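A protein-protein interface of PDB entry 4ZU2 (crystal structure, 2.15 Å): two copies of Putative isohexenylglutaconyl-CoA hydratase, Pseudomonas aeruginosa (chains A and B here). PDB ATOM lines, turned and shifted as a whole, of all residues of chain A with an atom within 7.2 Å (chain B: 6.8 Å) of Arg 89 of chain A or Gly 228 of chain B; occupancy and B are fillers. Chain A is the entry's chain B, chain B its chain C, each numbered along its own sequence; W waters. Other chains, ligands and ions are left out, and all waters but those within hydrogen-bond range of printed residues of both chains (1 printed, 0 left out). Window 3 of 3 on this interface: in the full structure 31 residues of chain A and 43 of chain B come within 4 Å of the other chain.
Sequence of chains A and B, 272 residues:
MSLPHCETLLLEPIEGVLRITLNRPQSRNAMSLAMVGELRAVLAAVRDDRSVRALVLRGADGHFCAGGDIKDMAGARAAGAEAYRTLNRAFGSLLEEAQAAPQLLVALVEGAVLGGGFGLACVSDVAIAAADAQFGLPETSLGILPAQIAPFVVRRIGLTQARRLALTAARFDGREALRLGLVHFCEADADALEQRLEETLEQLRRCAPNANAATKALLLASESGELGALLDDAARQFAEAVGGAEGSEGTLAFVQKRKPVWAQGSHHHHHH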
ATOM      1  N   VAL A  36       4.700 -11.206  23.187  1.00  0.00           N
ATOM      2  CA  VAL A  36       3.407 -10.561  23.359  1.00  0.00           C
ATOM      3  C   VAL A  36       2.577 -11.538  24.184  1.00  0.00           C
ATOM      4  O   VAL A  36       2.013 -11.168  25.204  1.00  0.00           O
ATOM      5  CB  VAL A  36       2.678 -10.226  22.003  1.00  0.00           C
ATOM      6  CG1 VAL A  36       1.201  -9.914  22.211  1.00  0.00           C
ATOM      7  CG2 VAL A  36       3.334  -9.070  21.308  1.00  0.00           C
ATOM      8  N   ARG A  40       1.540 -10.803  28.129  1.00  0.00           N
ATOM      9  CA  ARG A  40       0.128 -10.723  28.491  1.00  0.00           C
ATOM     10  C   ARG A  40      -0.264 -11.708  29.585  1.00  0.00           C
ATOM     11  O   ARG A  40      -1.243 -11.480  30.307  1.00  0.00           O
ATOM     12  CB  ARG A  40      -0.799 -10.955  27.285  1.00  0.00           C
ATOM     13  CG  ARG A  40      -0.736  -9.893  26.208  1.00  0.00           C
ATOM     14  CD  ARG A  40      -1.704 -10.174  25.072  1.00  0.00           C
ATOM     15  NE  ARG A  40      -3.074  -9.928  25.488  1.00  0.00           N
ATOM     16  CZ  ARG A  40      -4.151 -10.373  24.843  1.00  0.00           C
ATOM     17  NH1 ARG A  40      -4.008 -11.053  23.737  1.00  0.00           N
ATOM     18  NH2 ARG A  40      -5.379 -10.121  25.299  1.00  0.00           N
ATOM     19  N   ALA A  83      -4.550 -11.886   9.595  1.00  0.00           N
ATOM     20  CA  ALA A  83      -3.658 -12.362  10.650  1.00  0.00           C
ATOM     21  C   ALA A  83      -2.822 -11.211  11.185  1.00  0.00           C
ATOM     22  O   ALA A  83      -2.332 -11.267  12.311  1.00  0.00           O
ATOM     23  CB  ALA A  83      -2.760 -13.444  10.130  1.00  0.00           C
ATOM     24  N   TYR A  84      -2.651 -10.179  10.357  1.00  0.00           N
ATOM     25  CA  TYR A  84      -2.005  -8.935  10.769  1.00  0.00           C
ATOM     26  C   TYR A  84      -2.924  -8.097  11.666  1.00  0.00           C
ATOM     27  O   TYR A  84      -2.460  -7.432  12.591  1.00  0.00           O
ATOM     28  CB  TYR A  84      -1.584  -8.100   9.542  1.00  0.00           C
ATOM     29  CG  TYR A  84      -0.221  -8.451   8.981  1.00  0.00           C
ATOM     30  CD1 TYR A  84       0.935  -8.305   9.750  1.00  0.00           C
ATOM     31  CD2 TYR A  84      -0.084  -8.903   7.682  1.00  0.00           C
ATOM     32  CE1 TYR A  84       2.186  -8.620   9.239  1.00  0.00           C
ATOM     33  CE2 TYR A  84       1.158  -9.220   7.161  1.00  0.00           C
ATOM     34  CZ  TYR A  84       2.298  -9.086   7.939  1.00  0.00           C
ATOM     35  OH  TYR A  84       3.550  -9.394   7.428  1.00  0.00           O
ATOM     36  N   ARG A  85      -4.220  -8.119  11.378  1.00  0.00           N
ATOM     37  CA  ARG A  85      -5.189  -7.407  12.196  1.00  0.00           C
ATOM     38  C   ARG A  85      -5.136  -7.918  13.627  1.00  0.00           C
ATOM     39  O   ARG A  85      -4.797  -7.190  14.548  1.00  0.00           O
ATOM     40  CB  ARG A  85      -6.600  -7.623  11.663  1.00  0.00           C
ATOM     41  CG  ARG A  85      -7.639  -6.942  12.489  1.00  0.00           C
ATOM     42  CD  ARG A  85      -9.041  -7.122  11.931  1.00  0.00           C
ATOM     43  NE  ARG A  85      -9.961  -6.265  12.675  1.00  0.00           N
ATOM     44  CZ  ARG A  85     -11.169  -5.900  12.260  1.00  0.00           C
ATOM     45  NH1 ARG A  85     -11.632  -6.340  11.097  1.00  0.00           N
ATOM     46  NH2 ARG A  85     -11.920  -5.093  13.018  1.00  0.00           N
ATOM     47  N   THR A  86      -5.448  -9.194  13.782  1.00  0.00           N
ATOM     48  CA  THR A  86      -5.642  -9.784  15.090  1.00  0.00           C
ATOM     49  C   THR A  86      -4.319  -9.906  15.837  1.00  0.00           C
ATOM     50  O   THR A  86      -4.293  -9.978  17.078  1.00  0.00           O
ATOM     51  CB  THR A  86      -6.308 -11.152  14.948  1.00  0.00           C
ATOM     52  OG1 THR A  86      -5.568 -11.932  14.006  1.00  0.00           O
ATOM     53  CG2 THR A  86      -7.764 -10.989  14.448  1.00  0.00           C
ATOM     54  N   LEU A  87      -3.221  -9.919  15.091  1.00  0.00           N
ATOM     55  CA  LEU A  87      -1.901  -9.884  15.703  1.00  0.00           C
ATOM     56  C   LEU A  87      -1.655  -8.475  16.185  1.00  0.00           C
ATOM     57  O   LEU A  87      -1.234  -8.262  17.299  1.00  0.00           O
ATOM     58  CB  LEU A  87      -0.793 -10.278  14.718  1.00  0.00           C
ATOM     59  CG  LEU A  87      -0.255 -11.715  14.761  1.00  0.00           C
ATOM     60  CD1 LEU A  87      -1.362 -12.771  14.865  1.00  0.00           C
ATOM     61  CD2 LEU A  87       0.622 -11.967  13.540  1.00  0.00           C
ATOM     62  N   ASN A  88      -1.916  -7.508  15.322  1.00  0.00           N
ATOM     63  CA  ASN A  88      -1.768  -6.131  15.726  1.00  0.00           C
ATOM     64  C   ASN A  88      -2.618  -5.795  16.942  1.00  0.00           C
ATOM     65  O   ASN A  88      -2.119  -5.208  17.910  1.00  0.00           O
ATOM     66  CB  ASN A  88      -2.110  -5.212  14.574  1.00  0.00           C
ATOM     67  CG  ASN A  88      -1.699  -3.830  14.834  1.00  0.00           C
ATOM     68  OD1 ASN A  88      -2.505  -2.930  14.742  1.00  0.00           O
ATOM     69  ND2 ASN A  88      -0.422  -3.638  15.193  1.00  0.00           N
ATOM     70  N   ARG A  89      -3.886  -6.195  16.894  1.00  0.00           N
ATOM     71  CA  ARG A  89      -4.821  -5.948  17.983  1.00  0.00           C
ATOM     72  C   ARG A  89      -4.382  -6.619  19.295  1.00  0.00           C
ATOM     73  O   ARG A  89      -4.594  -6.073  20.370  1.00  0.00           O
ATOM     74  CB  ARG A  89      -6.227  -6.448  17.629  1.00  0.00           C
ATOM     75  CG  ARG A  89      -7.272  -6.119  18.704  1.00  0.00           C
ATOM     76  CD  ARG A  89      -7.411  -4.599  18.850  1.00  0.00           C
ATOM     77  NE  ARG A  89      -8.427  -4.164  19.805  1.00  0.00           N
ATOM     78  CZ  ARG A  89      -8.198  -3.909  21.092  1.00  0.00           C
ATOM     79  NH1 ARG A  89      -6.991  -4.071  21.606  1.00  0.00           N
ATOM     80  NH2 ARG A  89      -9.194  -3.511  21.875  1.00  0.00           N
ATOM     81  N   ALA A  90      -3.783  -7.802  19.190  1.00  0.00           N
ATOM     82  CA  ALA A  90      -3.307  -8.526  20.357  1.00  0.00           C
ATOM     83  C   ALA A  90      -2.139  -7.796  21.000  1.00  0.00           C
ATOM     84  O   ALA A  90      -1.913  -7.933  22.184  1.00  0.00           O
ATOM     85  CB  ALA A  90      -2.903  -9.963  19.970  1.00  0.00           C
ATOM     86  N   PHE A  91      -1.414  -7.005  20.218  1.00  0.00           N
ATOM     87  CA  PHE A  91      -0.356  -6.166  20.752  1.00  0.00           C
ATOM     88  C   PHE A  91      -0.983  -4.931  21.386  1.00  0.00           C
ATOM     89  O   PHE A  91      -0.493  -4.412  22.397  1.00  0.00           O
ATOM     90  CB  PHE A  91       0.651  -5.781  19.655  1.00  0.00           C
ATOM     91  CG  PHE A  91       1.507  -4.612  20.011  1.00  0.00           C
ATOM     92  CD1 PHE A  91       2.451  -4.708  21.027  1.00  0.00           C
ATOM     93  CD2 PHE A  91       1.349  -3.407  19.361  1.00  0.00           C
ATOM     94  CE1 PHE A  91       3.212  -3.626  21.381  1.00  0.00           C
ATOM     95  CE2 PHE A  91       2.117  -2.317  19.706  1.00  0.00           C
ATOM     96  CZ  PHE A  91       3.053  -2.431  20.725  1.00  0.00           C
ATOM     97  N   GLY A  92      -2.066  -4.471  20.771  1.00  0.00           N
ATOM     98  CA  GLY A  92      -2.912  -3.455  21.369  1.00  0.00           C
ATOM     99  C   GLY A  92      -3.346  -3.881  22.775  1.00  0.00           C
ATOM    100  O   GLY A  92      -3.235  -3.085  23.722  1.00  0.00           O
ATOM    101  N   SER A  93      -3.823  -5.127  22.911  1.00  0.00           N
ATOM    102  CA  SER A  93      -4.322  -5.639  24.191  1.00  0.00           C
ATOM    103  C   SER A  93      -3.242  -5.710  25.267  1.00  0.00           C
ATOM    104  O   SER A  93      -3.539  -5.613  26.451  1.00  0.00           O
ATOM    105  CB  SER A  93      -4.943  -7.024  24.028  1.00  0.00           C
ATOM    106  OG  SER A  93      -6.054  -6.958  23.164  1.00  0.00           O
ATOM    107  N   LEU A  94      -1.999  -5.892  24.848  1.00  0.00           N
ATOM    108  CA  LEU A  94      -0.877  -5.827  25.758  1.00  0.00           C
ATOM    109  C   LEU A  94      -0.736  -4.395  26.275  1.00  0.00           C
ATOM    110  O   LEU A  94      -0.536  -4.180  27.478  1.00  0.00           O
ATOM    111  CB  LEU A  94       0.411  -6.293  25.058  1.00  0.00           C
ATOM    112  CG  LEU A  94       1.738  -6.087  25.774  1.00  0.00           C
ATOM    113  CD1 LEU A  94       1.810  -6.956  27.057  1.00  0.00           C
ATOM    114  CD2 LEU A  94       2.918  -6.365  24.840  1.00  0.00           C
ATOM    115  N   LEU A  95      -0.839  -3.415  25.377  1.00  0.00           N
ATOM    116  CA  LEU A  95      -0.774  -2.029  25.819  1.00  0.00           C
ATOM    117  C   LEU A  95      -1.912  -1.700  26.797  1.00  0.00           C
ATOM    118  O   LEU A  95      -1.668  -1.019  27.794  1.00  0.00           O
ATOM    119  CB  LEU A  95      -0.685  -1.021  24.656  1.00  0.00           C
ATOM    120  CG  LEU A  95       0.604  -1.104  23.801  1.00  0.00           C
ATOM    121  CD1 LEU A  95       0.561  -0.182  22.583  1.00  0.00           C
ATOM    122  CD2 LEU A  95       1.875  -0.811  24.600  1.00  0.00           C
ATOM    123  N   GLU A  96      -3.118  -2.217  26.554  1.00  0.00           N
ATOM    124  CA  GLU A  96      -4.253  -1.941  27.448  1.00  0.00           C
ATOM    125  C   GLU A  96      -3.990  -2.556  28.853  1.00  0.00           C
ATOM    126  O   GLU A  96      -4.061  -1.878  29.870  1.00  0.00           O
ATOM    127  CB  GLU A  96      -5.570  -2.472  26.859  1.00  0.00           C
ATOM    128  CG  GLU A  96      -6.150  -1.620  25.714  1.00  0.00           C
ATOM    129  CD  GLU A  96      -7.385  -2.237  25.066  1.00  0.00           C
ATOM    130  OE1 GLU A  96      -7.247  -3.352  24.536  1.00  0.00           O
ATOM    131  OE2 GLU A  96      -8.493  -1.621  25.078  1.00  0.00           O
ATOM    132  N   GLN A 148      -1.616   0.930  17.074  1.00  0.00           N
ATOM    133  CA  GLN A 148      -2.050   0.682  18.464  1.00  0.00           C
ATOM    134  C   GLN A 148      -1.407   1.679  19.416  1.00  0.00           C
ATOM    135  O   GLN A 148      -2.011   2.063  20.416  1.00  0.00           O
ATOM    136  CB  GLN A 148      -1.731  -0.756  18.922  1.00  0.00           C
ATOM    137  CG  GLN A 148      -2.359  -1.867  18.097  1.00  0.00           C
ATOM    138  CD  GLN A 148      -3.890  -1.782  18.023  1.00  0.00           C
ATOM    139  OE1 GLN A 148      -4.623  -2.228  18.928  1.00  0.00           O
ATOM    140  NE2 GLN A 148      -4.373  -1.226  16.929  1.00  0.00           N
ATOM    141  N   GLY B 225     -12.099   9.461  22.049  1.00  0.00           N
ATOM    142  CA  GLY B 225     -12.674   8.479  21.153  1.00  0.00           C
ATOM    143  C   GLY B 225     -12.352   7.146  21.817  1.00  0.00           C
ATOM    144  O   GLY B 225     -11.176   6.806  21.970  1.00  0.00           O
ATOM    145  N   GLU B 226     -13.392   6.422  22.232  1.00  0.00           N
ATOM    146  CA  GLU B 226     -13.258   5.246  23.100  1.00  0.00           C
ATOM    147  C   GLU B 226     -12.195   4.218  22.673  1.00  0.00           C
ATOM    148  O   GLU B 226     -12.213   3.706  21.561  1.00  0.00           O
ATOM    149  CB  GLU B 226     -14.620   4.571  23.253  1.00  0.00           C
ATOM    150  CG  GLU B 226     -14.614   3.338  24.107  1.00  0.00           C
ATOM    151  CD  GLU B 226     -15.181   2.159  23.360  1.00  0.00           C
ATOM    152  OE1 GLU B 226     -16.353   2.275  22.924  1.00  0.00           O
ATOM    153  OE2 GLU B 226     -14.470   1.133  23.200  1.00  0.00           O
ATOM    154  N   LEU B 227     -11.312   3.898  23.616  1.00  0.00           N
ATOM    155  CA  LEU B 227     -10.073   3.185  23.359  1.00  0.00           C
ATOM    156  C   LEU B 227     -10.249   1.839  22.633  1.00  0.00           C
ATOM    157  O   LEU B 227      -9.596   1.567  21.618  1.00  0.00           O
ATOM    158  CB  LEU B 227      -9.324   3.004  24.686  1.00  0.00           C
ATOM    159  CG  LEU B 227      -7.862   2.529  24.696  1.00  0.00           C
ATOM    160  CD1 LEU B 227      -6.997   3.309  23.761  1.00  0.00           C
ATOM    161  CD2 LEU B 227      -7.311   2.627  26.109  1.00  0.00           C
ATOM    162  N   GLY B 228     -11.122   1.002  23.170  1.00  0.00           N
ATOM    163  CA  GLY B 228     -11.373  -0.312  22.609  1.00  0.00           C
ATOM    164  C   GLY B 228     -11.836  -0.296  21.167  1.00  0.00           C
ATOM    165  O   GLY B 228     -11.251  -0.975  20.350  1.00  0.00           O
ATOM    166  N   ALA B 229     -12.868   0.474  20.850  1.00  0.00           N
ATOM    167  CA  ALA B 229     -13.332   0.575  19.461  1.00  0.00           C
ATOM    168  C   ALA B 229     -12.231   1.090  18.514  1.00  0.00           C
ATOM    169  O   ALA B 229     -12.044   0.579  17.417  1.00  0.00           O
ATOM    170  CB  ALA B 229     -14.548   1.481  19.385  1.00  0.00           C
ATOM    171  N   LEU B 230     -11.506   2.095  18.982  1.00  0.00           N
ATOM    172  CA  LEU B 230     -10.461   2.746  18.243  1.00  0.00           C
ATOM    173  C   LEU B 230      -9.375   1.768  17.898  1.00  0.00           C
ATOM    174  O   LEU B 230      -8.883   1.740  16.774  1.00  0.00           O
ATOM    175  CB  LEU B 230      -9.891   3.876  19.089  1.00  0.00           C
ATOM    176  CG  LEU B 230      -8.827   4.800  18.509  1.00  0.00           C
ATOM    177  CD1 LEU B 230      -9.395   5.715  17.420  1.00  0.00           C
ATOM    178  CD2 LEU B 230      -8.241   5.616  19.593  1.00  0.00           C
ATOM    179  N   LEU B 231      -8.999   0.956  18.871  1.00  0.00           N
ATOM    180  CA  LEU B 231      -7.952  -0.028  18.646  1.00  0.00           C
ATOM    181  C   LEU B 231      -8.419  -1.087  17.660  1.00  0.00           C
ATOM    182  O   LEU B 231      -7.649  -1.515  16.795  1.00  0.00           O
ATOM    183  CB  LEU B 231      -7.479  -0.657  19.969  1.00  0.00           C
ATOM    184  CG  LEU B 231      -6.720   0.290  20.911  1.00  0.00           C
ATOM    185  CD1 LEU B 231      -6.450  -0.390  22.201  1.00  0.00           C
ATOM    186  CD2 LEU B 231      -5.411   0.774  20.316  1.00  0.00           C
ATOM    187  N   ASP B 232      -9.682  -1.492  17.767  1.00  0.00           N
ATOM    188  CA  ASP B 232     -10.230  -2.469  16.849  1.00  0.00           C
ATOM    189  C   ASP B 232     -10.048  -1.973  15.393  1.00  0.00           C
ATOM    190  O   ASP B 232      -9.528  -2.695  14.532  1.00  0.00           O
ATOM    191  CB  ASP B 232     -11.697  -2.737  17.165  1.00  0.00           C
ATOM    192  CG  ASP B 232     -11.881  -3.602  18.409  1.00  0.00           C
ATOM    193  OD1 ASP B 232     -10.876  -4.119  18.954  1.00  0.00           O
ATOM    194  OD2 ASP B 232     -13.040  -3.772  18.831  1.00  0.00           O
ATOM    195  N   ASP B 233     -10.457  -0.733  15.151  1.00  0.00           N
ATOM    196  CA  ASP B 233     -10.429  -0.148  13.834  1.00  0.00           C
ATOM    197  C   ASP B 233      -8.987   0.105  13.373  1.00  0.00           C
ATOM    198  O   ASP B 233      -8.609  -0.316  12.308  1.00  0.00           O
ATOM    199  CB  ASP B 233     -11.261   1.132  13.832  1.00  0.00           C
ATOM    200  CG  ASP B 233     -10.915   2.055  12.678  1.00  0.00           C
ATOM    201  OD1 ASP B 233     -11.220   1.718  11.516  1.00  0.00           O
ATOM    202  OD2 ASP B 233     -10.354   3.134  12.938  1.00  0.00           O
ATOM    203  N   ALA B 235      -6.498  -1.474  14.048  1.00  0.00           N
ATOM    204  CA  ALA B 235      -5.853  -2.726  13.753  1.00  0.00           C
ATOM    205  C   ALA B 235      -6.261  -3.176  12.347  1.00  0.00           C
ATOM    206  O   ALA B 235      -5.459  -3.759  11.643  1.00  0.00           O
ATOM    207  CB  ALA B 235      -6.196  -3.754  14.775  1.00  0.00           C
ATOM    208  N   PHE B 238      -4.133  -1.106  10.181  1.00  0.00           N
ATOM    209  CA  PHE B 238      -2.756  -1.562  10.217  1.00  0.00           C
ATOM    210  C   PHE B 238      -2.529  -2.689   9.197  1.00  0.00           C
ATOM    211  O   PHE B 238      -1.511  -2.727   8.522  1.00  0.00           O
ATOM    212  CB  PHE B 238      -2.376  -2.035  11.618  1.00  0.00           C
ATOM    213  CG  PHE B 238      -0.992  -2.582  11.700  1.00  0.00           C
ATOM    214  CD1 PHE B 238       0.095  -1.737  11.802  1.00  0.00           C
ATOM    215  CD2 PHE B 238      -0.771  -3.935  11.646  1.00  0.00           C
ATOM    216  CE1 PHE B 238       1.385  -2.244  11.858  1.00  0.00           C
ATOM    217  CE2 PHE B 238       0.510  -4.447  11.705  1.00  0.00           C
ATOM    218  CZ  PHE B 238       1.591  -3.600  11.816  1.00  0.00           C
HETATM  219  O   HOH W   1     -11.551  -4.141  21.623  1.00  0.00           O
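NE2 of Gln 148 of chain A lies within hydrogen-bond range of O of Leu 231 of chain B (3.3 Å). The side-chain carboxylate of Asp 232 of chain B lies within salt-bridge range of the guanidinium group of Arg 89 of chain A, 2.6 Å away.
Of the 17 printed residues of chain A, 6 touch a printed residue of chain B. Along chain A the printed residues that touch a printed residue of chain B span positions 84 to 148. Of the 11 printed residues of chain B, 5 touch a printed residue of chain A. Hydrophobic or aromatic side chains of chain B within 4 Å of the printed part of chain A: Leu 231, Ala 235 and Phe 238. Along chain B the printed residues that touch a printed residue of chain A span positions 228 to 238. Among the printed residues, 12 pairs touch across the chains.
No position is printed for both chains. Of the 12 pairs that touch across the chains among the printed residues, none has its exchanged pair printed and touching as well.
Printed residues of chain B within 4 Å of Tyr 84 of chain A: Phe 238. Printed residues of chain B within 4 Å of Asn 88 of chain A: Ala 235 (3.5 Å) and Phe 238 (3.3 Å). Arg 89 of chain A touches four residues of chain B. Of the printed residues of chain B, Glu 96 of chain A touches Leu 231 (3.5 Å). Of the printed residues of chain A, Gly 228 of chain B touches Arg 89. Of the printed residues of chain A, Asp 232 of chain B touches Arg 85 and Arg 89. Of the printed residues of chain A, Phe 238 of chain B touches Tyr 84 (3.997 Å) and Asn 88 (3.3 Å). The nearest printed residue of chain A that does not touch Gly 228 of chain B is Glu 96 of chain A (4.01 Å). The nearest printed residue of chain B that does not touch Glu 96 of chain A is Gly 228 of chain B (4.01 Å).
Tyr 84 of chain A touches Phe 238 of chain B. NH2 of Arg 85 of chain A touches O of Asp 232 of chain B, at 3.7 Å. Arg 85 of chain A touches Ala 235 of chain B (CA to O, 3.7 Å). OD1 of Asn 88 of chain A touches CA of Ala 235 of chain B, 3.5 Å away. Phe 238 of chain B touches Asn 88 of chain A. Arg 89 of chain A touches Gly 228 of chain B (NH2 to O, 3.6 Å). Arg 89 of chain A touches Leu 231 of chain B. Arg 89 of chain A touches Ala 235 of chain B. Leu 231 of chain B touches Glu 96 of chain A (CD1 to CD, 3.5 Å). NE2 of Gln 148 of chain A touches N of Ala 235 of chain B (3.6 Å).
Water W1 lies within hydrogen-bond range of NH2 of Arg 89 of chain A (2.5 Å), OD1 of Asp 232 of chain B (2.8 Å) and O of Gly 228 of chain B (3.4 Å).
The side-chain amide oxygen (OD1) of Asn 88 of chain A is in hydrogen-bond range of the side-chain amide nitrogen (NE2) of Gln 148 of chain A. The backbone carbonyl oxygen (O) of Arg 89 of chain A sits at hydrogen-bond distance from the side-chain hydroxyl (OG) of Ser 93 of chain A (3.3 Å). NH1 of Arg 89 of chain A is in salt-bridge range of OE1 of Glu 96 of chain A, 3.0 Å away. N of Gly 228 of chain B lies within hydrogen-bond range of OE2 of Glu 226 of chain B (3.4 Å).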
